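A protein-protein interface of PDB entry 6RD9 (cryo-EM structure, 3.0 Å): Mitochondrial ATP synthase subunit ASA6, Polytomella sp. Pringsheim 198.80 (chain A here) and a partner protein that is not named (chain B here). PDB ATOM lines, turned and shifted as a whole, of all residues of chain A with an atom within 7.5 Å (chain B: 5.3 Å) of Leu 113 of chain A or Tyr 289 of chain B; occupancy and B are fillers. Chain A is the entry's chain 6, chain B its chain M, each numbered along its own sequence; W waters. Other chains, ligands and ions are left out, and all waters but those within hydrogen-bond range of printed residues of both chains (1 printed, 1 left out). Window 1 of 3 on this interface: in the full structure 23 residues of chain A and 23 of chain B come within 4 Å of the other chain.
Leu 113 of chain A touches just these residues of chain B: Pro 169 and Tyr 289.
Of chain A, only Trp 112, Leu 113 and Phe 116 come within 4 Å of Tyr 289 of chain B.
Of the printed residues of chain A, Met 168 of chain B touches Gln 109 (3.0 Å).
Printed residues of chain A within 4 Å of Leu 167 of chain B: Gln 109 (3.5 Å).
The nearest printed residue of chain B that does not touch Leu 113 of chain A is Leu 167 of chain B (4.04 Å).
Water W1 bridges the side-chain amide nitrogen of Gln 109 of chain A and the side-chain carboxylate of Glu 288 of chain B.
Of the 13 printed residues of chain B, 6 touch a printed residue of chain A.
Hydrophobic or aromatic side chains of chain B that line the printed part of chain A: Pro 169, Val 285 and Tyr 289.
Hydrophobic or aromatic side chains of chain A within 4 Å of the printed part of chain B: Trp 112, Leu 113 and Phe 116.
Along chain A the printed residues that touch a printed residue of chain B span positions 109 to 116.
O of Met 168 of chain B lies close to OE1 of Gln 109 of chain A (3.0 Å).
Among the printed residues, pairs that only touch across the chains: Gln 109 of chain A with Leu 167 of chain B (3.5 Å), Gln 109 of chain A with Pro 169 of chain B (3.3 Å), Trp 112 of chain A with Val 285 of chain B (3.6 Å), Trp 112 of chain A with Gly 286 of chain B (3.6 Å), Trp 112 of chain A with Tyr 289 of chain B (3.8 Å), Leu 113 of chain A with Pro 169 of chain B (3.98 Å), Leu 113 of chain A with Tyr 289 of chain B (3.4 Å) and Phe 116 of chain A with Tyr 289 of chain B (3.5 Å).
OG of Ser 117 of chain A is in hydrogen-bond range of O of Leu 113 of chain A.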
ATOM      1  N   VAL A 107       5.746  -0.016   6.536  1.00  0.00           N
ATOM      2  CA  VAL A 107       6.307   0.724   5.416  1.00  0.00           C
ATOM      3  C   VAL A 107       5.224   1.049   4.405  1.00  0.00           C
ATOM      4  O   VAL A 107       5.225   2.122   3.801  1.00  0.00           O
ATOM      5  CB  VAL A 107       7.456  -0.090   4.799  1.00  0.00           C
ATOM      6  CG1 VAL A 107       8.052   0.610   3.628  1.00  0.00           C
ATOM      7  CG2 VAL A 107       8.506  -0.326   5.824  1.00  0.00           C
ATOM      8  N   LEU A 108       4.263   0.152   4.230  1.00  0.00           N
ATOM      9  CA  LEU A 108       3.159   0.420   3.323  1.00  0.00           C
ATOM     10  C   LEU A 108       2.202   1.441   3.889  1.00  0.00           C
ATOM     11  O   LEU A 108       1.607   2.212   3.139  1.00  0.00           O
ATOM     12  CB  LEU A 108       2.400  -0.858   3.032  1.00  0.00           C
ATOM     13  CG  LEU A 108       2.861  -1.667   1.851  1.00  0.00           C
ATOM     14  CD1 LEU A 108       2.033  -2.890   1.808  1.00  0.00           C
ATOM     15  CD2 LEU A 108       2.620  -0.851   0.643  1.00  0.00           C
ATOM     16  N   GLN A 109       2.019   1.442   5.199  1.00  0.00           N
ATOM     17  CA  GLN A 109       1.103   2.379   5.815  1.00  0.00           C
ATOM     18  C   GLN A 109       1.708   3.761   5.935  1.00  0.00           C
ATOM     19  O   GLN A 109       0.997   4.750   5.769  1.00  0.00           O
ATOM     20  CB  GLN A 109       0.688   1.867   7.180  1.00  0.00           C
ATOM     21  CG  GLN A 109      -0.235   0.721   7.109  1.00  0.00           C
ATOM     22  CD  GLN A 109      -0.294  -0.020   8.392  1.00  0.00           C
ATOM     23  OE1 GLN A 109       0.467   0.241   9.301  1.00  0.00           O
ATOM     24  NE2 GLN A 109      -1.214  -0.954   8.487  1.00  0.00           N
ATOM     25  N   ALA A 110       3.005   3.857   6.218  1.00  0.00           N
ATOM     26  CA  ALA A 110       3.667   5.147   6.278  1.00  0.00           C
ATOM     27  C   ALA A 110       3.972   5.717   4.915  1.00  0.00           C
ATOM     28  O   ALA A 110       4.399   6.864   4.830  1.00  0.00           O
ATOM     29  CB  ALA A 110       4.968   5.060   7.057  1.00  0.00           C
ATOM     30  N   ALA A 111       3.805   4.947   3.854  1.00  0.00           N
ATOM     31  CA  ALA A 111       3.994   5.500   2.527  1.00  0.00           C
ATOM     32  C   ALA A 111       2.825   6.378   2.143  1.00  0.00           C
ATOM     33  O   ALA A 111       2.971   7.283   1.322  1.00  0.00           O
ATOM     34  CB  ALA A 111       4.173   4.384   1.512  1.00  0.00           C
ATOM     35  N   TRP A 112       1.650   6.112   2.705  1.00  0.00           N
ATOM     36  CA  TRP A 112       0.473   6.919   2.431  1.00  0.00           C
ATOM     37  C   TRP A 112       0.394   8.145   3.305  1.00  0.00           C
ATOM     38  O   TRP A 112      -0.239   9.119   2.916  1.00  0.00           O
ATOM     39  CB  TRP A 112      -0.782   6.094   2.618  1.00  0.00           C
ATOM     40  CG  TRP A 112      -1.161   5.388   1.420  1.00  0.00           C
ATOM     41  CD1 TRP A 112      -0.934   4.097   1.147  1.00  0.00           C
ATOM     42  CD2 TRP A 112      -1.827   5.930   0.292  1.00  0.00           C
ATOM     43  NE1 TRP A 112      -1.419   3.781  -0.084  1.00  0.00           N
ATOM     44  CE2 TRP A 112      -1.976   4.899  -0.632  1.00  0.00           C
ATOM     45  CE3 TRP A 112      -2.306   7.191  -0.030  1.00  0.00           C
ATOM     46  CZ2 TRP A 112      -2.585   5.084  -1.855  1.00  0.00           C
ATOM     47  CZ3 TRP A 112      -2.914   7.373  -1.238  1.00  0.00           C
ATOM     48  CH2 TRP A 112      -3.052   6.327  -2.138  1.00  0.00           C
ATOM     49  N   LEU A 113       1.002   8.116   4.481  1.00  0.00           N
ATOM     50  CA  LEU A 113       1.150   9.323   5.273  1.00  0.00           C
ATOM     51  C   LEU A 113       2.081  10.309   4.599  1.00  0.00           C
ATOM     52  O   LEU A 113       1.961  11.516   4.804  1.00  0.00           O
ATOM     53  CB  LEU A 113       1.678   8.968   6.653  1.00  0.00           C
ATOM     54  CG  LEU A 113       0.740   8.734   7.822  1.00  0.00           C
ATOM     55  CD1 LEU A 113      -0.130   7.584   7.569  1.00  0.00           C
ATOM     56  CD2 LEU A 113       1.589   8.424   9.001  1.00  0.00           C
ATOM     57  N   ILE A 114       3.028   9.813   3.818  1.00  0.00           N
ATOM     58  CA  ILE A 114       3.925  10.671   3.063  1.00  0.00           C
ATOM     59  C   ILE A 114       3.226  11.205   1.824  1.00  0.00           C
ATOM     60  O   ILE A 114       3.364  12.378   1.475  1.00  0.00           O
ATOM     61  CB  ILE A 114       5.202   9.876   2.744  1.00  0.00           C
ATOM     62  CG1 ILE A 114       6.103   9.858   3.967  1.00  0.00           C
ATOM     63  CG2 ILE A 114       5.915  10.390   1.538  1.00  0.00           C
ATOM     64  CD1 ILE A 114       7.058   8.750   3.969  1.00  0.00           C
ATOM     65  N   SER A 115       2.435  10.369   1.163  1.00  0.00           N
ATOM     66  CA  SER A 115       1.735  10.806  -0.030  1.00  0.00           C
ATOM     67  C   SER A 115       0.539  11.677   0.284  1.00  0.00           C
ATOM     68  O   SER A 115      -0.009  12.296  -0.624  1.00  0.00           O
ATOM     69  CB  SER A 115       1.285   9.610  -0.841  1.00  0.00           C
ATOM     70  OG  SER A 115       2.408   8.892  -1.291  1.00  0.00           O
ATOM     71  N   PHE A 116       0.101  11.720   1.535  1.00  0.00           N
ATOM     72  CA  PHE A 116      -0.969  12.627   1.911  1.00  0.00           C
ATOM     73  C   PHE A 116      -0.443  14.005   2.253  1.00  0.00           C
ATOM     74  O   PHE A 116      -1.162  14.987   2.091  1.00  0.00           O
ATOM     75  CB  PHE A 116      -1.746  12.059   3.084  1.00  0.00           C
ATOM     76  CG  PHE A 116      -2.771  11.059   2.687  1.00  0.00           C
ATOM     77  CD1 PHE A 116      -3.287  11.050   1.416  1.00  0.00           C
ATOM     78  CD2 PHE A 116      -3.213  10.121   3.584  1.00  0.00           C
ATOM     79  CE1 PHE A 116      -4.232  10.130   1.058  1.00  0.00           C
ATOM     80  CE2 PHE A 116      -4.143   9.201   3.221  1.00  0.00           C
ATOM     81  CZ  PHE A 116      -4.659   9.208   1.960  1.00  0.00           C
ATOM     82  N   SER A 117       0.803  14.109   2.696  1.00  0.00           N
ATOM     83  CA  SER A 117       1.407  15.416   2.882  1.00  0.00           C
ATOM     84  C   SER A 117       1.741  16.088   1.569  1.00  0.00           C
ATOM     85  O   SER A 117       2.011  17.287   1.552  1.00  0.00           O
ATOM     86  CB  SER A 117       2.676  15.294   3.701  1.00  0.00           C
ATOM     87  OG  SER A 117       2.439  14.527   4.855  1.00  0.00           O
ATOM     88  N   SER A 118       1.748  15.347   0.475  1.00  0.00           N
ATOM     89  CA  SER A 118       2.149  15.866  -0.810  1.00  0.00           C
ATOM     90  C   SER A 118       1.015  15.940  -1.805  1.00  0.00           C
ATOM     91  O   SER A 118       1.246  16.331  -2.949  1.00  0.00           O
ATOM     92  CB  SER A 118       3.270  15.005  -1.392  1.00  0.00           C
ATOM     93  OG  SER A 118       4.522  15.376  -0.843  1.00  0.00           O
ATOM     94  N   ILE A 120      -2.689  16.367  -0.552  1.00  0.00           N
ATOM     95  CA  ILE A 120      -3.881  17.024  -0.022  1.00  0.00           C
ATOM     96  C   ILE A 120      -3.714  18.529  -0.168  1.00  0.00           C
ATOM     97  O   ILE A 120      -2.681  19.071   0.251  1.00  0.00           O
ATOM     98  CB  ILE A 120      -4.096  16.638   1.432  1.00  0.00           C
ATOM     99  CG1 ILE A 120      -4.410  15.160   1.543  1.00  0.00           C
ATOM    100  CG2 ILE A 120      -5.249  17.398   2.000  1.00  0.00           C
ATOM    101  CD1 ILE A 120      -4.531  14.686   2.952  1.00  0.00           C
ATOM    102  N   PHE A 122      -3.937  21.632   1.337  1.00  0.00           N
ATOM    103  CA  PHE A 122      -4.217  21.933   2.727  1.00  0.00           C
ATOM    104  C   PHE A 122      -4.834  23.298   2.927  1.00  0.00           C
ATOM    105  O   PHE A 122      -5.417  23.543   3.979  1.00  0.00           O
ATOM    106  CB  PHE A 122      -2.950  21.825   3.545  1.00  0.00           C
ATOM    107  CG  PHE A 122      -2.539  20.438   3.810  1.00  0.00           C
ATOM    108  CD1 PHE A 122      -3.257  19.654   4.675  1.00  0.00           C
ATOM    109  CD2 PHE A 122      -1.426  19.911   3.206  1.00  0.00           C
ATOM    110  CE1 PHE A 122      -2.874  18.375   4.929  1.00  0.00           C
ATOM    111  CE2 PHE A 122      -1.040  18.636   3.464  1.00  0.00           C
ATOM    112  CZ  PHE A 122      -1.765  17.868   4.326  1.00  0.00           C
ATOM    113  N   LEU B 164      -9.236   4.335  11.279  1.00  0.00           N
ATOM    114  CA  LEU B 164      -8.040   4.971  10.775  1.00  0.00           C
ATOM    115  C   LEU B 164      -6.821   4.688  11.621  1.00  0.00           C
ATOM    116  O   LEU B 164      -5.723   5.026  11.192  1.00  0.00           O
ATOM    117  CB  LEU B 164      -8.223   6.477  10.680  1.00  0.00           C
ATOM    118  CG  LEU B 164      -9.125   7.087   9.619  1.00  0.00           C
ATOM    119  CD1 LEU B 164      -9.110   8.557   9.825  1.00  0.00           C
ATOM    120  CD2 LEU B 164      -8.694   6.753   8.237  1.00  0.00           C
ATOM    121  N   LEU B 167      -4.607   2.174   9.763  1.00  0.00           N
ATOM    122  CA  LEU B 167      -3.802   2.703   8.682  1.00  0.00           C
ATOM    123  C   LEU B 167      -2.637   3.537   9.175  1.00  0.00           C
ATOM    124  O   LEU B 167      -1.859   4.024   8.362  1.00  0.00           O
ATOM    125  CB  LEU B 167      -4.686   3.524   7.763  1.00  0.00           C
ATOM    126  CG  LEU B 167      -5.873   2.682   7.361  1.00  0.00           C
ATOM    127  CD1 LEU B 167      -6.952   3.575   6.950  1.00  0.00           C
ATOM    128  CD2 LEU B 167      -5.470   1.822   6.218  1.00  0.00           C
ATOM    129  N   MET B 168      -2.515   3.729  10.456  1.00  0.00           N
ATOM    130  CA  MET B 168      -1.296   4.279  10.999  1.00  0.00           C
ATOM    131  C   MET B 168      -0.267   3.171  11.136  1.00  0.00           C
ATOM    132  O   MET B 168      -0.625   2.025  11.386  1.00  0.00           O
ATOM    133  CB  MET B 168      -1.547   4.916  12.355  1.00  0.00           C
ATOM    134  CG  MET B 168      -2.489   6.075  12.326  1.00  0.00           C
ATOM    135  SD  MET B 168      -2.007   7.315  11.135  1.00  0.00           S
ATOM    136  CE  MET B 168      -3.372   7.249   9.990  1.00  0.00           C
ATOM    137  N   PRO B 169       1.006   3.473  10.933  1.00  0.00           N
ATOM    138  CA  PRO B 169       2.034   2.457  11.127  1.00  0.00           C
ATOM    139  C   PRO B 169       2.150   2.045  12.579  1.00  0.00           C
ATOM    140  O   PRO B 169       1.882   2.827  13.487  1.00  0.00           O
ATOM    141  CB  PRO B 169       3.304   3.145  10.632  1.00  0.00           C
ATOM    142  CG  PRO B 169       2.980   4.541  10.550  1.00  0.00           C
ATOM    143  CD  PRO B 169       1.553   4.648  10.252  1.00  0.00           C
ATOM    144  N   VAL B 285      -3.784  -0.301   0.179  1.00  0.00           N
ATOM    145  CA  VAL B 285      -3.803   0.562   1.347  1.00  0.00           C
ATOM    146  C   VAL B 285      -4.605   1.814   1.051  1.00  0.00           C
ATOM    147  O   VAL B 285      -5.231   2.383   1.945  1.00  0.00           O
ATOM    148  CB  VAL B 285      -2.372   0.887   1.797  1.00  0.00           C
ATOM    149  CG1 VAL B 285      -2.367   1.529   3.159  1.00  0.00           C
ATOM    150  CG2 VAL B 285      -1.589  -0.352   1.861  1.00  0.00           C
ATOM    151  N   GLY B 286      -4.628   2.253  -0.201  1.00  0.00           N
ATOM    152  CA  GLY B 286      -5.445   3.395  -0.552  1.00  0.00           C
ATOM    153  C   GLY B 286      -6.921   3.091  -0.562  1.00  0.00           C
ATOM    154  O   GLY B 286      -7.731   3.954  -0.242  1.00  0.00           O
ATOM    155  N   LEU B 287      -7.294   1.876  -0.941  1.00  0.00           N
ATOM    156  CA  LEU B 287      -8.687   1.473  -0.838  1.00  0.00           C
ATOM    157  C   LEU B 287      -9.090   1.295   0.612  1.00  0.00           C
ATOM    158  O   LEU B 287     -10.250   1.505   0.966  1.00  0.00           O
ATOM    159  CB  LEU B 287      -8.904   0.185  -1.625  1.00  0.00           C
ATOM    160  CG  LEU B 287     -10.205  -0.597  -1.512  1.00  0.00           C
ATOM    161  CD1 LEU B 287     -11.337   0.253  -1.973  1.00  0.00           C
ATOM    162  CD2 LEU B 287     -10.129  -1.846  -2.330  1.00  0.00           C
ATOM    163  N   GLU B 288      -8.141   0.937   1.463  1.00  0.00           N
ATOM    164  CA  GLU B 288      -8.427   0.774   2.875  1.00  0.00           C
ATOM    165  C   GLU B 288      -8.664   2.096   3.573  1.00  0.00           C
ATOM    166  O   GLU B 288      -9.278   2.120   4.636  1.00  0.00           O
ATOM    167  CB  GLU B 288      -7.279   0.059   3.543  1.00  0.00           C
ATOM    168  CG  GLU B 288      -7.351  -1.407   3.464  1.00  0.00           C
ATOM    169  CD  GLU B 288      -6.268  -2.015   4.276  1.00  0.00           C
ATOM    170  OE1 GLU B 288      -5.984  -1.506   5.375  1.00  0.00           O
ATOM    171  OE2 GLU B 288      -5.678  -2.997   3.810  1.00  0.00           O
ATOM    172  N   TYR B 289      -8.142   3.192   3.031  1.00  0.00           N
ATOM    173  CA  TYR B 289      -8.493   4.503   3.552  1.00  0.00           C
ATOM    174  C   TYR B 289      -9.897   4.882   3.160  1.00  0.00           C
ATOM    175  O   TYR B 289     -10.516   5.720   3.807  1.00  0.00           O
ATOM    176  CB  TYR B 289      -7.546   5.559   3.025  1.00  0.00           C
ATOM    177  CG  TYR B 289      -6.346   5.803   3.860  1.00  0.00           C
ATOM    178  CD1 TYR B 289      -6.388   6.687   4.906  1.00  0.00           C
ATOM    179  CD2 TYR B 289      -5.162   5.161   3.585  1.00  0.00           C
ATOM    180  CE1 TYR B 289      -5.287   6.918   5.662  1.00  0.00           C
ATOM    181  CE2 TYR B 289      -4.062   5.380   4.337  1.00  0.00           C
ATOM    182  CZ  TYR B 289      -4.125   6.261   5.369  1.00  0.00           C
ATOM    183  OH  TYR B 289      -3.014   6.483   6.124  1.00  0.00           O
ATOM    184  N   LEU B 290     -10.387   4.327   2.069  1.00  0.00           N
ATOM    185  CA  LEU B 290     -11.739   4.605   1.632  1.00  0.00           C
ATOM    186  C   LEU B 290     -12.734   3.756   2.390  1.00  0.00           C
ATOM    187  O   LEU B 290     -13.816   4.224   2.728  1.00  0.00           O
ATOM    188  CB  LEU B 290     -11.843   4.354   0.138  1.00  0.00           C
ATOM    189  CG  LEU B 290     -12.919   5.084  -0.637  1.00  0.00           C
ATOM    190  CD1 LEU B 290     -12.821   6.555  -0.373  1.00  0.00           C
ATOM    191  CD2 LEU B 290     -12.707   4.797  -2.086  1.00  0.00           C
ATOM    192  N   VAL B 291     -12.370   2.516   2.695  1.00  0.00           N
ATOM    193  CA  VAL B 291     -13.237   1.638   3.465  1.00  0.00           C
ATOM    194  C   VAL B 291     -13.252   2.041   4.936  1.00  0.00           C
ATOM    195  O   VAL B 291     -14.256   1.858   5.625  1.00  0.00           O
ATOM    196  CB  VAL B 291     -12.773   0.195   3.211  1.00  0.00           C
ATOM    197  CG1 VAL B 291     -13.419  -0.798   4.115  1.00  0.00           C
ATOM    198  CG2 VAL B 291     -13.085  -0.169   1.791  1.00  0.00           C
ATOM    199  N   ALA B 292     -12.177   2.651   5.428  1.00  0.00           N
ATOM    200  CA  ALA B 292     -12.153   3.149   6.797  1.00  0.00           C
ATOM    201  C   ALA B 292     -13.120   4.298   6.992  1.00  0.00           C
ATOM    202  O   ALA B 292     -13.746   4.410   8.046  1.00  0.00           O
ATOM    203  CB  ALA B 292     -10.748   3.598   7.164  1.00  0.00           C
ATOM    204  N   VAL B 293     -13.260   5.157   5.992  1.00  0.00           N
ATOM    205  CA  VAL B 293     -14.159   6.294   6.094  1.00  0.00           C
ATOM    206  C   VAL B 293     -15.574   5.893   5.723  1.00  0.00           C
ATOM    207  O   VAL B 293     -16.537   6.398   6.296  1.00  0.00           O
ATOM    208  CB  VAL B 293     -13.628   7.444   5.224  1.00  0.00           C
ATOM    209  CG1 VAL B 293     -14.490   8.666   5.323  1.00  0.00           C
ATOM    210  CG2 VAL B 293     -12.249   7.802   5.651  1.00  0.00           C
HETATM  211  O   HOH W   1      -2.994  -0.792   6.126  1.00  0.00           O
